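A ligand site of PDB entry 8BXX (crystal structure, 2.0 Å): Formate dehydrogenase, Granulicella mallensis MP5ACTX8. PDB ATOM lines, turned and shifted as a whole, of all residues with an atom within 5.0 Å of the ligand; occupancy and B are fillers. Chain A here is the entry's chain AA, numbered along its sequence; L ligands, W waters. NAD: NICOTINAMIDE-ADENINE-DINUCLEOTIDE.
Water W2 bridges O2A of the ligand and NH1 of Arg 202.
Water W3 lies within hydrogen-bond range of the backbone carbonyl oxygen (O) of Asn 255 (2.8 Å), an oxygen (O2N) of the ligand (2.8 Å), the backbone NH (N) of Gly 204 (3.0 Å) and the backbone NH (N) of Gly 201 (3.1 Å).
Water W4 lies within hydrogen-bond range of the side-chain carboxylate of Asp 126 (2.7 Å), an oxygen (O2D) of the ligand (2.8 Å) and the backbone NH of Leu 258 (3.0 Å).
O2A of the ligand is in salt-bridge range of NH1 of Arg 202 (2.9 Å).
OD1 of Asp 222 is in hydrogen-bond range of O2B of the ligand (2.7 Å).
An oxygen (O1N) of the ligand is in hydrogen-bond range of the side-chain hydroxyl (OG) of Ser 148 (2.8 Å).
The side-chain hydroxyl (OG) of Ser 335 sits at hydrogen-bond distance from an oxygen (O7N) of the ligand, 3.2 Å away.
NE2 of His 333 sits at hydrogen-bond distance from N7N of the ligand, 3.1 Å away.
NE2 of His 259 sits close to N7A of the ligand (3.4 Å).
The backbone NH (N) of Ile 203 lies within hydrogen-bond range of an oxygen (O2N) of the ligand, 2.9 Å away.
N of Arg 202 sits at hydrogen-bond distance from O2A of the ligand, 3.0 Å away.
The backbone NH (N) of His 259 lies within hydrogen-bond range of the side-chain hydroxyl (OG1) of Thr 262 (3.1 Å).
The backbone NH of Asn 255 is in hydrogen-bond range of the backbone carbonyl oxygen of Val 198 (2.8 Å).
The backbone NH (N) of His 224 is in hydrogen-bond range of the side-chain carboxylate (OD1) of Asp 222 (2.8 Å).
The side-chain hydroxyl (OG1) of Thr 262 sits at hydrogen-bond distance from the backbone carbonyl oxygen (O) of Pro 257 (2.6 Å).
The backbone NH (N) of Ala 200 is in hydrogen-bond range of the side-chain carboxylate (OD2) of Asp 222, at 2.7 Å.
The side-chain carboxylate (OD2) of Asp 309 is in hydrogen-bond range of the side-chain hydroxyl (OG) of Ser 335.
The backbone carbonyl oxygen (O) of Phe 221 sits at hydrogen-bond distance from the backbone NH (N) of Ala 199 (2.8 Å).
The guanidinium group (NH2) of Arg 285 sits at hydrogen-bond distance from the backbone carbonyl oxygen (O) of Ile 123 (2.9 Å).
An oxygen (O7N) of the ligand lies close to the backbone carbonyl oxygen of Thr 283 (2.9 Å).
OD2 of Asp 309 sits close to O7N of the ligand, 3.0 Å away.
A nitrogen (N7N) of the ligand sits close to the backbone NH (N) of Gly 336 (2.8 Å).
CE1 of Phe 99 touches N7N of the ligand, 3.5 Å away.
CB of Ile 123 touches C5N of the ligand (3.7 Å).
CA of Gly 124 touches O3D of the ligand, at 3.9 Å.
Asn 147 touches the ligand.
CG2 of Val 151 touches C4N of the ligand (3.3 Å).
CG1 of Val 198 touches C2A of the ligand (3.9 Å).
CB of Ala 199 touches O4B of the ligand, 3.3 Å away.
Gly 201 touches the ligand.
Phe 221 touches the ligand.
OE1 of Gln 223 touches N7A of the ligand (3.5 Å).
CD2 of His 224 touches O2B of the ligand (3.7 Å).
Asn 255 touches the ligand.
Ala 256 touches the ligand (CB to C4A, 3.8 Å).
Pro 257 touches the ligand.
CG2 of Thr 262 touches N6A of the ligand (3.4 Å).
Ala 284 touches the ligand (O to C1D, 3.5 Å).
Arg 285 touches the ligand.
Val 310 touches the ligand (CG1 to O7N, 3.9 Å).
The nearest printed residue that does not touch the ligand is Ala 200 (4.2 Å).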
ATOM      1  N   PHE A  99      28.902 -16.156  -9.706  1.00  0.00           N
ATOM      2  CA  PHE A  99      28.684 -16.775 -11.009  1.00  0.00           C
ATOM      3  C   PHE A  99      29.682 -16.240 -12.036  1.00  0.00           C
ATOM      4  O   PHE A  99      29.904 -16.878 -13.078  1.00  0.00           O
ATOM      5  CB  PHE A  99      27.246 -16.557 -11.497  1.00  0.00           C
ATOM      6  CG  PHE A  99      26.304 -16.544 -10.332  1.00  0.00           C
ATOM      7  CD1 PHE A  99      26.078 -17.712  -9.605  1.00  0.00           C
ATOM      8  CD2 PHE A  99      25.787 -15.346  -9.848  1.00  0.00           C
ATOM      9  CE1 PHE A  99      25.296 -17.690  -8.455  1.00  0.00           C
ATOM     10  CE2 PHE A  99      24.984 -15.338  -8.715  1.00  0.00           C
ATOM     11  CZ  PHE A  99      24.775 -16.496  -8.008  1.00  0.00           C
ATOM     12  N   ILE A 123      26.122 -15.576  -2.497  1.00  0.00           N
ATOM     13  CA  ILE A 123      26.570 -16.179  -1.242  1.00  0.00           C
ATOM     14  C   ILE A 123      27.916 -16.861  -1.473  1.00  0.00           C
ATOM     15  O   ILE A 123      28.099 -17.510  -2.503  1.00  0.00           O
ATOM     16  CB  ILE A 123      25.507 -17.158  -0.725  1.00  0.00           C
ATOM     17  CG1 ILE A 123      24.139 -16.457  -0.534  1.00  0.00           C
ATOM     18  CG2 ILE A 123      25.981 -17.890   0.525  1.00  0.00           C
ATOM     19  CD1 ILE A 123      22.985 -17.357  -0.078  1.00  0.00           C
ATOM     20  N   GLY A 124      28.821 -16.769  -0.489  1.00  0.00           N
ATOM     21  CA  GLY A 124      30.093 -17.494  -0.595  1.00  0.00           C
ATOM     22  C   GLY A 124      31.185 -16.564  -1.112  1.00  0.00           C
ATOM     23  O   GLY A 124      31.246 -16.278  -2.305  1.00  0.00           O
ATOM     24  N   ASP A 126      34.546 -16.837  -1.209  1.00  0.00           N
ATOM     25  CA  ASP A 126      35.818 -17.541  -1.293  1.00  0.00           C
ATOM     26  C   ASP A 126      36.721 -16.874  -2.335  1.00  0.00           C
ATOM     27  O   ASP A 126      37.943 -17.126  -2.365  1.00  0.00           O
ATOM     28  CB  ASP A 126      35.576 -19.041  -1.534  1.00  0.00           C
ATOM     29  CG  ASP A 126      34.515 -19.295  -2.621  1.00  0.00           C
ATOM     30  OD1 ASP A 126      33.288 -19.215  -2.329  1.00  0.00           O
ATOM     31  OD2 ASP A 126      34.909 -19.518  -3.756  1.00  0.00           O
ATOM     32  N   ASN A 147      19.960 -16.802  -2.084  1.00  0.00           N
ATOM     33  CA  ASN A 147      19.682 -17.825  -3.094  1.00  0.00           C
ATOM     34  C   ASN A 147      19.770 -19.241  -2.504  1.00  0.00           C
ATOM     35  O   ASN A 147      19.721 -20.202  -3.256  1.00  0.00           O
ATOM     36  CB  ASN A 147      20.536 -17.652  -4.351  1.00  0.00           C
ATOM     37  CG  ASN A 147      22.013 -17.631  -4.008  1.00  0.00           C
ATOM     38  OD1 ASN A 147      22.389 -18.106  -2.943  1.00  0.00           O
ATOM     39  ND2 ASN A 147      22.861 -17.084  -4.866  1.00  0.00           N
ATOM     40  N   SER A 148      19.875 -19.374  -1.173  1.00  0.00           N
ATOM     41  CA  SER A 148      20.005 -20.696  -0.577  1.00  0.00           C
ATOM     42  C   SER A 148      18.883 -21.644  -1.026  1.00  0.00           C
ATOM     43  O   SER A 148      19.098 -22.849  -1.191  1.00  0.00           O
ATOM     44  CB  SER A 148      20.065 -20.619   0.938  1.00  0.00           C
ATOM     45  OG  SER A 148      21.023 -19.676   1.361  1.00  0.00           O
ATOM     46  N   VAL A 151      19.219 -22.878  -4.624  1.00  0.00           N
ATOM     47  CA  VAL A 151      20.182 -23.969  -4.732  1.00  0.00           C
ATOM     48  C   VAL A 151      19.541 -25.299  -4.341  1.00  0.00           C
ATOM     49  O   VAL A 151      19.721 -26.283  -5.053  1.00  0.00           O
ATOM     50  CB  VAL A 151      21.460 -23.674  -3.919  1.00  0.00           C
ATOM     51  CG1 VAL A 151      22.502 -24.773  -4.114  1.00  0.00           C
ATOM     52  CG2 VAL A 151      22.087 -22.337  -4.299  1.00  0.00           C
ATOM     53  N   VAL A 198      26.512 -33.000   3.201  1.00  0.00           N
ATOM     54  CA  VAL A 198      27.617 -32.340   3.870  1.00  0.00           C
ATOM     55  C   VAL A 198      27.159 -30.914   4.139  1.00  0.00           C
ATOM     56  O   VAL A 198      27.028 -30.141   3.198  1.00  0.00           O
ATOM     57  CB  VAL A 198      28.904 -32.351   3.024  1.00  0.00           C
ATOM     58  CG1 VAL A 198      30.057 -31.692   3.788  1.00  0.00           C
ATOM     59  CG2 VAL A 198      29.285 -33.759   2.614  1.00  0.00           C
ATOM     60  N   ALA A 199      26.963 -30.604   5.427  1.00  0.00           N
ATOM     61  CA  ALA A 199      26.487 -29.334   5.965  1.00  0.00           C
ATOM     62  C   ALA A 199      24.966 -29.357   6.030  1.00  0.00           C
ATOM     63  O   ALA A 199      24.289 -29.909   5.148  1.00  0.00           O
ATOM     64  CB  ALA A 199      27.029 -28.146   5.185  1.00  0.00           C
ATOM     65  N   ALA A 200      24.442 -28.801   7.115  1.00  0.00           N
ATOM     66  CA  ALA A 200      23.017 -28.504   7.242  1.00  0.00           C
ATOM     67  C   ALA A 200      22.834 -27.036   7.617  1.00  0.00           C
ATOM     68  O   ALA A 200      22.049 -26.723   8.522  1.00  0.00           O
ATOM     69  CB  ALA A 200      22.353 -29.442   8.241  1.00  0.00           C
ATOM     70  N   GLY A 201      23.457 -26.128   6.862  1.00  0.00           N
ATOM     71  CA  GLY A 201      23.181 -24.696   6.940  1.00  0.00           C
ATOM     72  C   GLY A 201      21.929 -24.327   6.137  1.00  0.00           C
ATOM     73  O   GLY A 201      21.007 -25.107   6.029  1.00  0.00           O
ATOM     74  N   ARG A 202      21.902 -23.116   5.585  1.00  0.00           N
ATOM     75  CA  ARG A 202      20.698 -22.661   4.922  1.00  0.00           C
ATOM     76  C   ARG A 202      20.353 -23.562   3.733  1.00  0.00           C
ATOM     77  O   ARG A 202      19.186 -23.960   3.588  1.00  0.00           O
ATOM     78  CB  ARG A 202      20.813 -21.177   4.571  1.00  0.00           C
ATOM     79  CG  ARG A 202      20.825 -20.312   5.821  1.00  0.00           C
ATOM     80  CD  ARG A 202      21.301 -18.889   5.577  1.00  0.00           C
ATOM     81  NE  ARG A 202      21.319 -18.063   6.790  1.00  0.00           N
ATOM     82  CZ  ARG A 202      22.369 -17.852   7.548  1.00  0.00           C
ATOM     83  NH1 ARG A 202      23.535 -18.411   7.273  1.00  0.00           N
ATOM     84  NH2 ARG A 202      22.272 -17.042   8.579  1.00  0.00           N
ATOM     85  N   ILE A 203      21.348 -23.903   2.900  1.00  0.00           N
ATOM     86  CA  ILE A 203      21.064 -24.787   1.774  1.00  0.00           C
ATOM     87  C   ILE A 203      20.781 -26.222   2.246  1.00  0.00           C
ATOM     88  O   ILE A 203      19.758 -26.807   1.886  1.00  0.00           O
ATOM     89  CB  ILE A 203      22.166 -24.727   0.690  1.00  0.00           C
ATOM     90  CG1 ILE A 203      22.222 -23.329   0.065  1.00  0.00           C
ATOM     91  CG2 ILE A 203      21.909 -25.786  -0.373  1.00  0.00           C
ATOM     92  CD1 ILE A 203      23.434 -23.070  -0.825  1.00  0.00           C
ATOM     93  N   GLY A 204      21.691 -26.785   3.048  1.00  0.00           N
ATOM     94  CA  GLY A 204      21.614 -28.176   3.451  1.00  0.00           C
ATOM     95  C   GLY A 204      20.312 -28.511   4.180  1.00  0.00           C
ATOM     96  O   GLY A 204      19.705 -29.559   3.914  1.00  0.00           O
ATOM     97  N   PHE A 221      26.340 -34.556   8.123  1.00  0.00           N
ATOM     98  CA  PHE A 221      27.348 -34.067   9.043  1.00  0.00           C
ATOM     99  C   PHE A 221      27.450 -32.554   8.879  1.00  0.00           C
ATOM    100  O   PHE A 221      27.425 -32.066   7.758  1.00  0.00           O
ATOM    101  CB  PHE A 221      28.738 -34.663   8.775  1.00  0.00           C
ATOM    102  CG  PHE A 221      29.839 -33.937   9.516  1.00  0.00           C
ATOM    103  CD1 PHE A 221      30.044 -34.155  10.871  1.00  0.00           C
ATOM    104  CD2 PHE A 221      30.622 -32.978   8.891  1.00  0.00           C
ATOM    105  CE1 PHE A 221      31.022 -33.455  11.580  1.00  0.00           C
ATOM    106  CE2 PHE A 221      31.595 -32.271   9.589  1.00  0.00           C
ATOM    107  CZ  PHE A 221      31.798 -32.512  10.939  1.00  0.00           C
ATOM    108  N   ASP A 222      27.650 -31.863  10.010  1.00  0.00           N
ATOM    109  CA  ASP A 222      27.919 -30.428  10.088  1.00  0.00           C
ATOM    110  C   ASP A 222      28.767 -30.166  11.335  1.00  0.00           C
ATOM    111  O   ASP A 222      28.556 -30.805  12.369  1.00  0.00           O
ATOM    112  CB  ASP A 222      26.617 -29.609  10.043  1.00  0.00           C
ATOM    113  CG  ASP A 222      26.819 -28.132   9.736  1.00  0.00           C
ATOM    114  OD1 ASP A 222      27.692 -27.501  10.395  1.00  0.00           O
ATOM    115  OD2 ASP A 222      26.108 -27.599   8.821  1.00  0.00           O
ATOM    116  N   GLN A 223      29.723 -29.223  11.225  1.00  0.00           N
ATOM    117  CA  GLN A 223      30.512 -28.825  12.380  1.00  0.00           C
ATOM    118  C   GLN A 223      29.593 -28.271  13.477  1.00  0.00           C
ATOM    119  O   GLN A 223      29.863 -28.444  14.659  1.00  0.00           O
ATOM    120  CB  GLN A 223      31.604 -27.800  12.005  1.00  0.00           C
ATOM    121  CG  GLN A 223      32.514 -28.207  10.836  1.00  0.00           C
ATOM    122  CD  GLN A 223      33.452 -27.087  10.414  1.00  0.00           C
ATOM    123  OE1 GLN A 223      33.089 -25.907  10.361  1.00  0.00           O
ATOM    124  NE2 GLN A 223      34.691 -27.453  10.103  1.00  0.00           N
ATOM    125  N   HIS A 224      28.483 -27.632  13.099  1.00  0.00           N
ATOM    126  CA  HIS A 224      27.482 -27.187  14.064  1.00  0.00           C
ATOM    127  C   HIS A 224      26.282 -28.118  13.952  1.00  0.00           C
ATOM    128  O   HIS A 224      25.551 -28.088  12.966  1.00  0.00           O
ATOM    129  CB  HIS A 224      27.089 -25.715  13.834  1.00  0.00           C
ATOM    130  CG  HIS A 224      28.194 -24.715  13.989  1.00  0.00           C
ATOM    131  ND1 HIS A 224      28.968 -24.640  15.132  1.00  0.00           N
ATOM    132  CD2 HIS A 224      28.640 -23.740  13.162  1.00  0.00           C
ATOM    133  CE1 HIS A 224      29.867 -23.664  14.997  1.00  0.00           C
ATOM    134  NE2 HIS A 224      29.680 -23.104  13.800  1.00  0.00           N
ATOM    135  N   VAL A 242      32.337 -36.638   7.737  1.00  0.00           N
ATOM    136  CA  VAL A 242      31.921 -36.866   6.364  1.00  0.00           C
ATOM    137  C   VAL A 242      32.204 -38.332   6.007  1.00  0.00           C
ATOM    138  O   VAL A 242      31.336 -39.030   5.501  1.00  0.00           O
ATOM    139  CB  VAL A 242      32.631 -35.889   5.396  1.00  0.00           C
ATOM    140  CG1 VAL A 242      32.171 -36.112   3.965  1.00  0.00           C
ATOM    141  CG2 VAL A 242      32.390 -34.446   5.818  1.00  0.00           C
ATOM    142  N   ASN A 255      27.020 -29.223   0.564  1.00  0.00           N
ATOM    143  CA  ASN A 255      26.426 -27.898   0.749  1.00  0.00           C
ATOM    144  C   ASN A 255      27.187 -27.057   1.769  1.00  0.00           C
ATOM    145  O   ASN A 255      26.583 -26.207   2.458  1.00  0.00           O
ATOM    146  CB  ASN A 255      24.937 -27.994   1.142  1.00  0.00           C
ATOM    147  CG  ASN A 255      24.143 -28.769   0.107  1.00  0.00           C
ATOM    148  OD1 ASN A 255      23.924 -28.280  -1.012  1.00  0.00           O
ATOM    149  ND2 ASN A 255      23.770 -30.000   0.455  1.00  0.00           N
ATOM    150  N   ALA A 256      28.507 -27.258   1.843  1.00  0.00           N
ATOM    151  CA  ALA A 256      29.378 -26.497   2.724  1.00  0.00           C
ATOM    152  C   ALA A 256      30.148 -25.434   1.928  1.00  0.00           C
ATOM    153  O   ALA A 256      30.333 -25.565   0.715  1.00  0.00           O
ATOM    154  CB  ALA A 256      30.349 -27.435   3.399  1.00  0.00           C
ATOM    155  N   PRO A 257      30.638 -24.361   2.582  1.00  0.00           N
ATOM    156  CA  PRO A 257      31.461 -23.360   1.893  1.00  0.00           C
ATOM    157  C   PRO A 257      32.839 -23.921   1.571  1.00  0.00           C
ATOM    158  O   PRO A 257      33.248 -24.922   2.181  1.00  0.00           O
ATOM    159  CB  PRO A 257      31.603 -22.257   2.956  1.00  0.00           C
ATOM    160  CG  PRO A 257      30.488 -22.525   3.939  1.00  0.00           C
ATOM    161  CD  PRO A 257      30.432 -24.041   3.989  1.00  0.00           C
ATOM    162  N   LEU A 258      33.522 -23.297   0.596  1.00  0.00           N
ATOM    163  CA  LEU A 258      34.921 -23.588   0.295  1.00  0.00           C
ATOM    164  C   LEU A 258      35.808 -22.879   1.315  1.00  0.00           C
ATOM    165  O   LEU A 258      35.846 -21.640   1.356  1.00  0.00           O
ATOM    166  CB  LEU A 258      35.319 -23.138  -1.122  1.00  0.00           C
ATOM    167  CG  LEU A 258      36.803 -23.309  -1.467  1.00  0.00           C
ATOM    168  CD1 LEU A 258      37.238 -24.762  -1.352  1.00  0.00           C
ATOM    169  CD2 LEU A 258      37.154 -22.780  -2.873  1.00  0.00           C
ATOM    170  N   HIS A 259      36.498 -23.692   2.112  1.00  0.00           N
ATOM    171  CA  HIS A 259      37.516 -23.232   3.045  1.00  0.00           C
ATOM    172  C   HIS A 259      38.458 -24.390   3.384  1.00  0.00           C
ATOM    173  O   HIS A 259      38.303 -25.494   2.870  1.00  0.00           O
ATOM    174  CB  HIS A 259      36.896 -22.435   4.214  1.00  0.00           C
ATOM    175  CG  HIS A 259      36.001 -23.176   5.141  1.00  0.00           C
ATOM    176  ND1 HIS A 259      35.995 -24.554   5.248  1.00  0.00           N
ATOM    177  CD2 HIS A 259      35.119 -22.728   6.062  1.00  0.00           C
ATOM    178  CE1 HIS A 259      35.121 -24.936   6.172  1.00  0.00           C
ATOM    179  NE2 HIS A 259      34.574 -23.826   6.693  1.00  0.00           N
ATOM    180  N   GLY A 261      39.042 -26.832   5.495  1.00  0.00           N
ATOM    181  CA  GLY A 261      38.464 -28.160   5.740  1.00  0.00           C
ATOM    182  C   GLY A 261      37.694 -28.797   4.576  1.00  0.00           C
ATOM    183  O   GLY A 261      37.430 -29.988   4.654  1.00  0.00           O
ATOM    184  N   THR A 262      37.322 -28.034   3.516  1.00  0.00           N
ATOM    185  CA  THR A 262      36.538 -28.583   2.397  1.00  0.00           C
ATOM    186  C   THR A 262      37.334 -28.653   1.091  1.00  0.00           C
ATOM    187  O   THR A 262      36.942 -29.356   0.160  1.00  0.00           O
ATOM    188  CB  THR A 262      35.162 -27.897   2.246  1.00  0.00           C
ATOM    189  OG1 THR A 262      35.286 -26.501   1.896  1.00  0.00           O
ATOM    190  CG2 THR A 262      34.291 -28.062   3.461  1.00  0.00           C
ATOM    191  N   THR A 283      26.635 -28.514  -5.585  1.00  0.00           N
ATOM    192  CA  THR A 283      26.303 -27.152  -5.942  1.00  0.00           C
ATOM    193  C   THR A 283      26.968 -26.159  -4.969  1.00  0.00           C
ATOM    194  O   THR A 283      26.545 -24.998  -4.861  1.00  0.00           O
ATOM    195  CB  THR A 283      24.782 -26.959  -5.864  1.00  0.00           C
ATOM    196  OG1 THR A 283      24.372 -27.412  -4.562  1.00  0.00           O
ATOM    197  CG2 THR A 283      24.055 -27.774  -6.910  1.00  0.00           C
ATOM    198  N   ALA A 284      28.003 -26.602  -4.248  1.00  0.00           N
ATOM    199  CA  ALA A 284      28.683 -25.757  -3.278  1.00  0.00           C
ATOM    200  C   ALA A 284      29.794 -24.959  -3.962  1.00  0.00           C
ATOM    201  O   ALA A 284      29.592 -23.803  -4.332  1.00  0.00           O
ATOM    202  CB  ALA A 284      29.147 -26.601  -2.087  1.00  0.00           C
ATOM    203  N   ARG A 285      30.982 -25.563  -4.077  1.00  0.00           N
ATOM    204  CA  ARG A 285      32.065 -25.006  -4.894  1.00  0.00           C
ATOM    205  C   ARG A 285      32.766 -26.155  -5.595  1.00  0.00           C
ATOM    206  O   ARG A 285      32.866 -27.243  -5.034  1.00  0.00           O
ATOM    207  CB  ARG A 285      33.070 -24.208  -4.026  1.00  0.00           C
ATOM    208  CG  ARG A 285      32.595 -22.826  -3.561  1.00  0.00           C
ATOM    209  CD  ARG A 285      32.295 -21.830  -4.668  1.00  0.00           C
ATOM    210  NE  ARG A 285      31.808 -20.509  -4.245  1.00  0.00           N
ATOM    211  CZ  ARG A 285      30.530 -20.111  -4.258  1.00  0.00           C
ATOM    212  NH1 ARG A 285      29.564 -20.922  -4.710  1.00  0.00           N
ATOM    213  NH2 ARG A 285      30.219 -18.861  -3.900  1.00  0.00           N
ATOM    214  N   ASP A 309      26.619 -27.403 -10.362  1.00  0.00           N
ATOM    215  CA  ASP A 309      26.684 -26.240 -11.215  1.00  0.00           C
ATOM    216  C   ASP A 309      28.035 -25.538 -11.059  1.00  0.00           C
ATOM    217  O   ASP A 309      28.268 -24.540 -11.718  1.00  0.00           O
ATOM    218  CB  ASP A 309      25.478 -25.312 -10.972  1.00  0.00           C
ATOM    219  CG  ASP A 309      25.417 -24.769  -9.551  1.00  0.00           C
ATOM    220  OD1 ASP A 309      25.941 -25.503  -8.616  1.00  0.00           O
ATOM    221  OD2 ASP A 309      24.848 -23.627  -9.370  1.00  0.00           O
ATOM    222  N   VAL A 310      28.939 -26.065 -10.204  1.00  0.00           N
ATOM    223  CA  VAL A 310      30.110 -25.293  -9.784  1.00  0.00           C
ATOM    224  C   VAL A 310      31.375 -25.976 -10.302  1.00  0.00           C
ATOM    225  O   VAL A 310      31.490 -27.198 -10.269  1.00  0.00           O
ATOM    226  CB  VAL A 310      30.157 -25.044  -8.260  1.00  0.00           C
ATOM    227  CG1 VAL A 310      29.214 -23.934  -7.797  1.00  0.00           C
ATOM    228  CG2 VAL A 310      29.957 -26.317  -7.433  1.00  0.00           C
ATOM    229  N   HIS A 333      27.389 -22.386 -13.849  1.00  0.00           N
ATOM    230  CA  HIS A 333      27.118 -21.941 -12.484  1.00  0.00           C
ATOM    231  C   HIS A 333      25.900 -21.012 -12.498  1.00  0.00           C
ATOM    232  O   HIS A 333      26.052 -19.801 -12.727  1.00  0.00           O
ATOM    233  CB  HIS A 333      28.382 -21.312 -11.874  1.00  0.00           C
ATOM    234  CG  HIS A 333      28.235 -20.910 -10.432  1.00  0.00           C
ATOM    235  ND1 HIS A 333      29.152 -20.097  -9.820  1.00  0.00           N
ATOM    236  CD2 HIS A 333      27.261 -21.152  -9.534  1.00  0.00           C
ATOM    237  CE1 HIS A 333      28.796 -19.874  -8.568  1.00  0.00           C
ATOM    238  NE2 HIS A 333      27.608 -20.513  -8.360  1.00  0.00           N
ATOM    239  N   ILE A 334      24.691 -21.590 -12.286  1.00  0.00           N
ATOM    240  CA  ILE A 334      23.461 -20.861 -12.560  1.00  0.00           C
ATOM    241  C   ILE A 334      22.471 -20.945 -11.407  1.00  0.00           C
ATOM    242  O   ILE A 334      21.502 -20.176 -11.405  1.00  0.00           O
ATOM    243  CB  ILE A 334      22.817 -21.319 -13.893  1.00  0.00           C
ATOM    244  CG1 ILE A 334      22.293 -22.758 -13.782  1.00  0.00           C
ATOM    245  CG2 ILE A 334      23.794 -21.129 -15.061  1.00  0.00           C
ATOM    246  CD1 ILE A 334      21.469 -23.230 -14.967  1.00  0.00           C
ATOM    247  N   SER A 335      22.633 -21.919 -10.484  1.00  0.00           N
ATOM    248  CA  SER A 335      21.534 -22.219  -9.565  1.00  0.00           C
ATOM    249  C   SER A 335      21.210 -20.991  -8.710  1.00  0.00           C
ATOM    250  O   SER A 335      20.040 -20.635  -8.546  1.00  0.00           O
ATOM    251  CB  SER A 335      21.694 -23.476  -8.734  1.00  0.00           C
ATOM    252  OG  SER A 335      22.708 -23.328  -7.756  1.00  0.00           O
ATOM    253  N   GLY A 336      22.259 -20.330  -8.213  1.00  0.00           N
ATOM    254  CA  GLY A 336      22.095 -19.177  -7.336  1.00  0.00           C
ATOM    255  C   GLY A 336      21.716 -17.919  -8.127  1.00  0.00           C
ATOM    256  O   GLY A 336      21.550 -16.857  -7.535  1.00  0.00           O
ATOM    257  N   THR A 337      21.575 -18.042  -9.454  1.00  0.00           N
ATOM    258  CA  THR A 337      21.267 -16.860 -10.264  1.00  0.00           C
ATOM    259  C   THR A 337      20.015 -17.056 -11.143  1.00  0.00           C
ATOM    260  O   THR A 337      19.898 -16.404 -12.178  1.00  0.00           O
ATOM    261  CB  THR A 337      22.524 -16.295 -10.941  1.00  0.00           C
ATOM    262  OG1 THR A 337      22.291 -14.935 -11.364  1.00  0.00           O
ATOM    263  CG2 THR A 337      23.022 -17.097 -12.118  1.00  0.00           C
HETATM  264  PA  NAD L   1      25.376 -21.275   5.462  1.00  0.00           P
HETATM  265  O1A NAD L   1      26.518 -20.488   6.006  1.00  0.00           O
HETATM  266  O2A NAD L   1      23.973 -20.953   5.858  1.00  0.00           O
HETATM  267  O5B NAD L   1      25.647 -22.834   5.649  1.00  0.00           O
HETATM  268  C5B NAD L   1      26.965 -23.414   5.488  1.00  0.00           C
HETATM  269  C4B NAD L   1      27.122 -24.527   6.495  1.00  0.00           C
HETATM  270  O4B NAD L   1      28.315 -25.294   6.236  1.00  0.00           O
HETATM  271  C3B NAD L   1      27.207 -24.124   7.983  1.00  0.00           C
HETATM  272  O3B NAD L   1      26.141 -24.717   8.724  1.00  0.00           O
HETATM  273  C2B NAD L   1      28.585 -24.650   8.426  1.00  0.00           C
HETATM  274  O2B NAD L   1      28.617 -25.097   9.770  1.00  0.00           O
HETATM  275  C1B NAD L   1      28.771 -25.812   7.461  1.00  0.00           C
HETATM  276  N9A NAD L   1      30.137 -26.307   7.287  1.00  0.00           N
HETATM  277  C8A NAD L   1      31.300 -25.596   7.085  1.00  0.00           C
HETATM  278  N7A NAD L   1      32.347 -26.371   6.925  1.00  0.00           N
HETATM  279  C5A NAD L   1      31.862 -27.656   6.999  1.00  0.00           C
HETATM  280  C6A NAD L   1      32.471 -28.925   6.898  1.00  0.00           C
HETATM  281  N6A NAD L   1      33.767 -29.120   6.698  1.00  0.00           N
HETATM  282  N1A NAD L   1      31.679 -30.010   7.029  1.00  0.00           N
HETATM  283  C2A NAD L   1      30.369 -29.839   7.193  1.00  0.00           C
HETATM  284  N3A NAD L   1      29.684 -28.706   7.306  1.00  0.00           N
HETATM  285  C4A NAD L   1      30.493 -27.639   7.191  1.00  0.00           C
HETATM  286  O3  NAD L   1      25.473 -21.102   3.872  1.00  0.00           O
HETATM  287  PN  NAD L   1      24.534 -21.588   2.659  1.00  0.00           P
HETATM  288  O1N NAD L   1      23.562 -20.502   2.297  1.00  0.00           O
HETATM  289  O2N NAD L   1      24.051 -22.940   3.088  1.00  0.00           O
HETATM  290  O5D NAD L   1      25.652 -21.673   1.500  1.00  0.00           O
HETATM  291  C5D NAD L   1      26.608 -22.788   1.589  1.00  0.00           C
HETATM  292  C4D NAD L   1      27.598 -22.638   0.461  1.00  0.00           C
HETATM  293  O4D NAD L   1      26.953 -22.985  -0.773  1.00  0.00           O
HETATM  294  C3D NAD L   1      28.130 -21.216   0.235  1.00  0.00           C
HETATM  295  O3D NAD L   1      29.268 -20.958   1.036  1.00  0.00           O
HETATM  296  C2D NAD L   1      28.534 -21.283  -1.247  1.00  0.00           C
HETATM  297  O2D NAD L   1      29.880 -21.737  -1.285  1.00  0.00           O
HETATM  298  C1D NAD L   1      27.562 -22.298  -1.864  1.00  0.00           C
HETATM  299  N1N NAD L   1      26.493 -21.652  -2.691  1.00  0.00           N
HETATM  300  C2N NAD L   1      26.368 -21.979  -4.020  1.00  0.00           C
HETATM  301  C3N NAD L   1      25.456 -21.310  -4.807  1.00  0.00           C
HETATM  302  C7N NAD L   1      25.297 -21.738  -6.231  1.00  0.00           C
HETATM  303  O7N NAD L   1      25.643 -22.890  -6.578  1.00  0.00           O
HETATM  304  N7N NAD L   1      24.783 -20.854  -7.048  1.00  0.00           N
HETATM  305  C4N NAD L   1      24.686 -20.258  -4.282  1.00  0.00           C
HETATM  306  C5N NAD L   1      24.772 -19.992  -2.928  1.00  0.00           C
HETATM  307  C6N NAD L   1      25.639 -20.733  -2.149  1.00  0.00           C
HETATM  308  O   HOH W   1      23.642 -17.858   3.218  1.00  0.00           O
HETATM  309  O   HOH W   2      23.585 -21.684   8.482  1.00  0.00           O
HETATM  310  O   HOH W   3      24.345 -25.604   3.942  1.00  0.00           O
HETATM  311  O   HOH W   4      32.296 -20.693  -0.267  1.00  0.00           O
HETATM  312  O   HOH W   5      34.658 -32.015   7.494  1.00  0.00           O
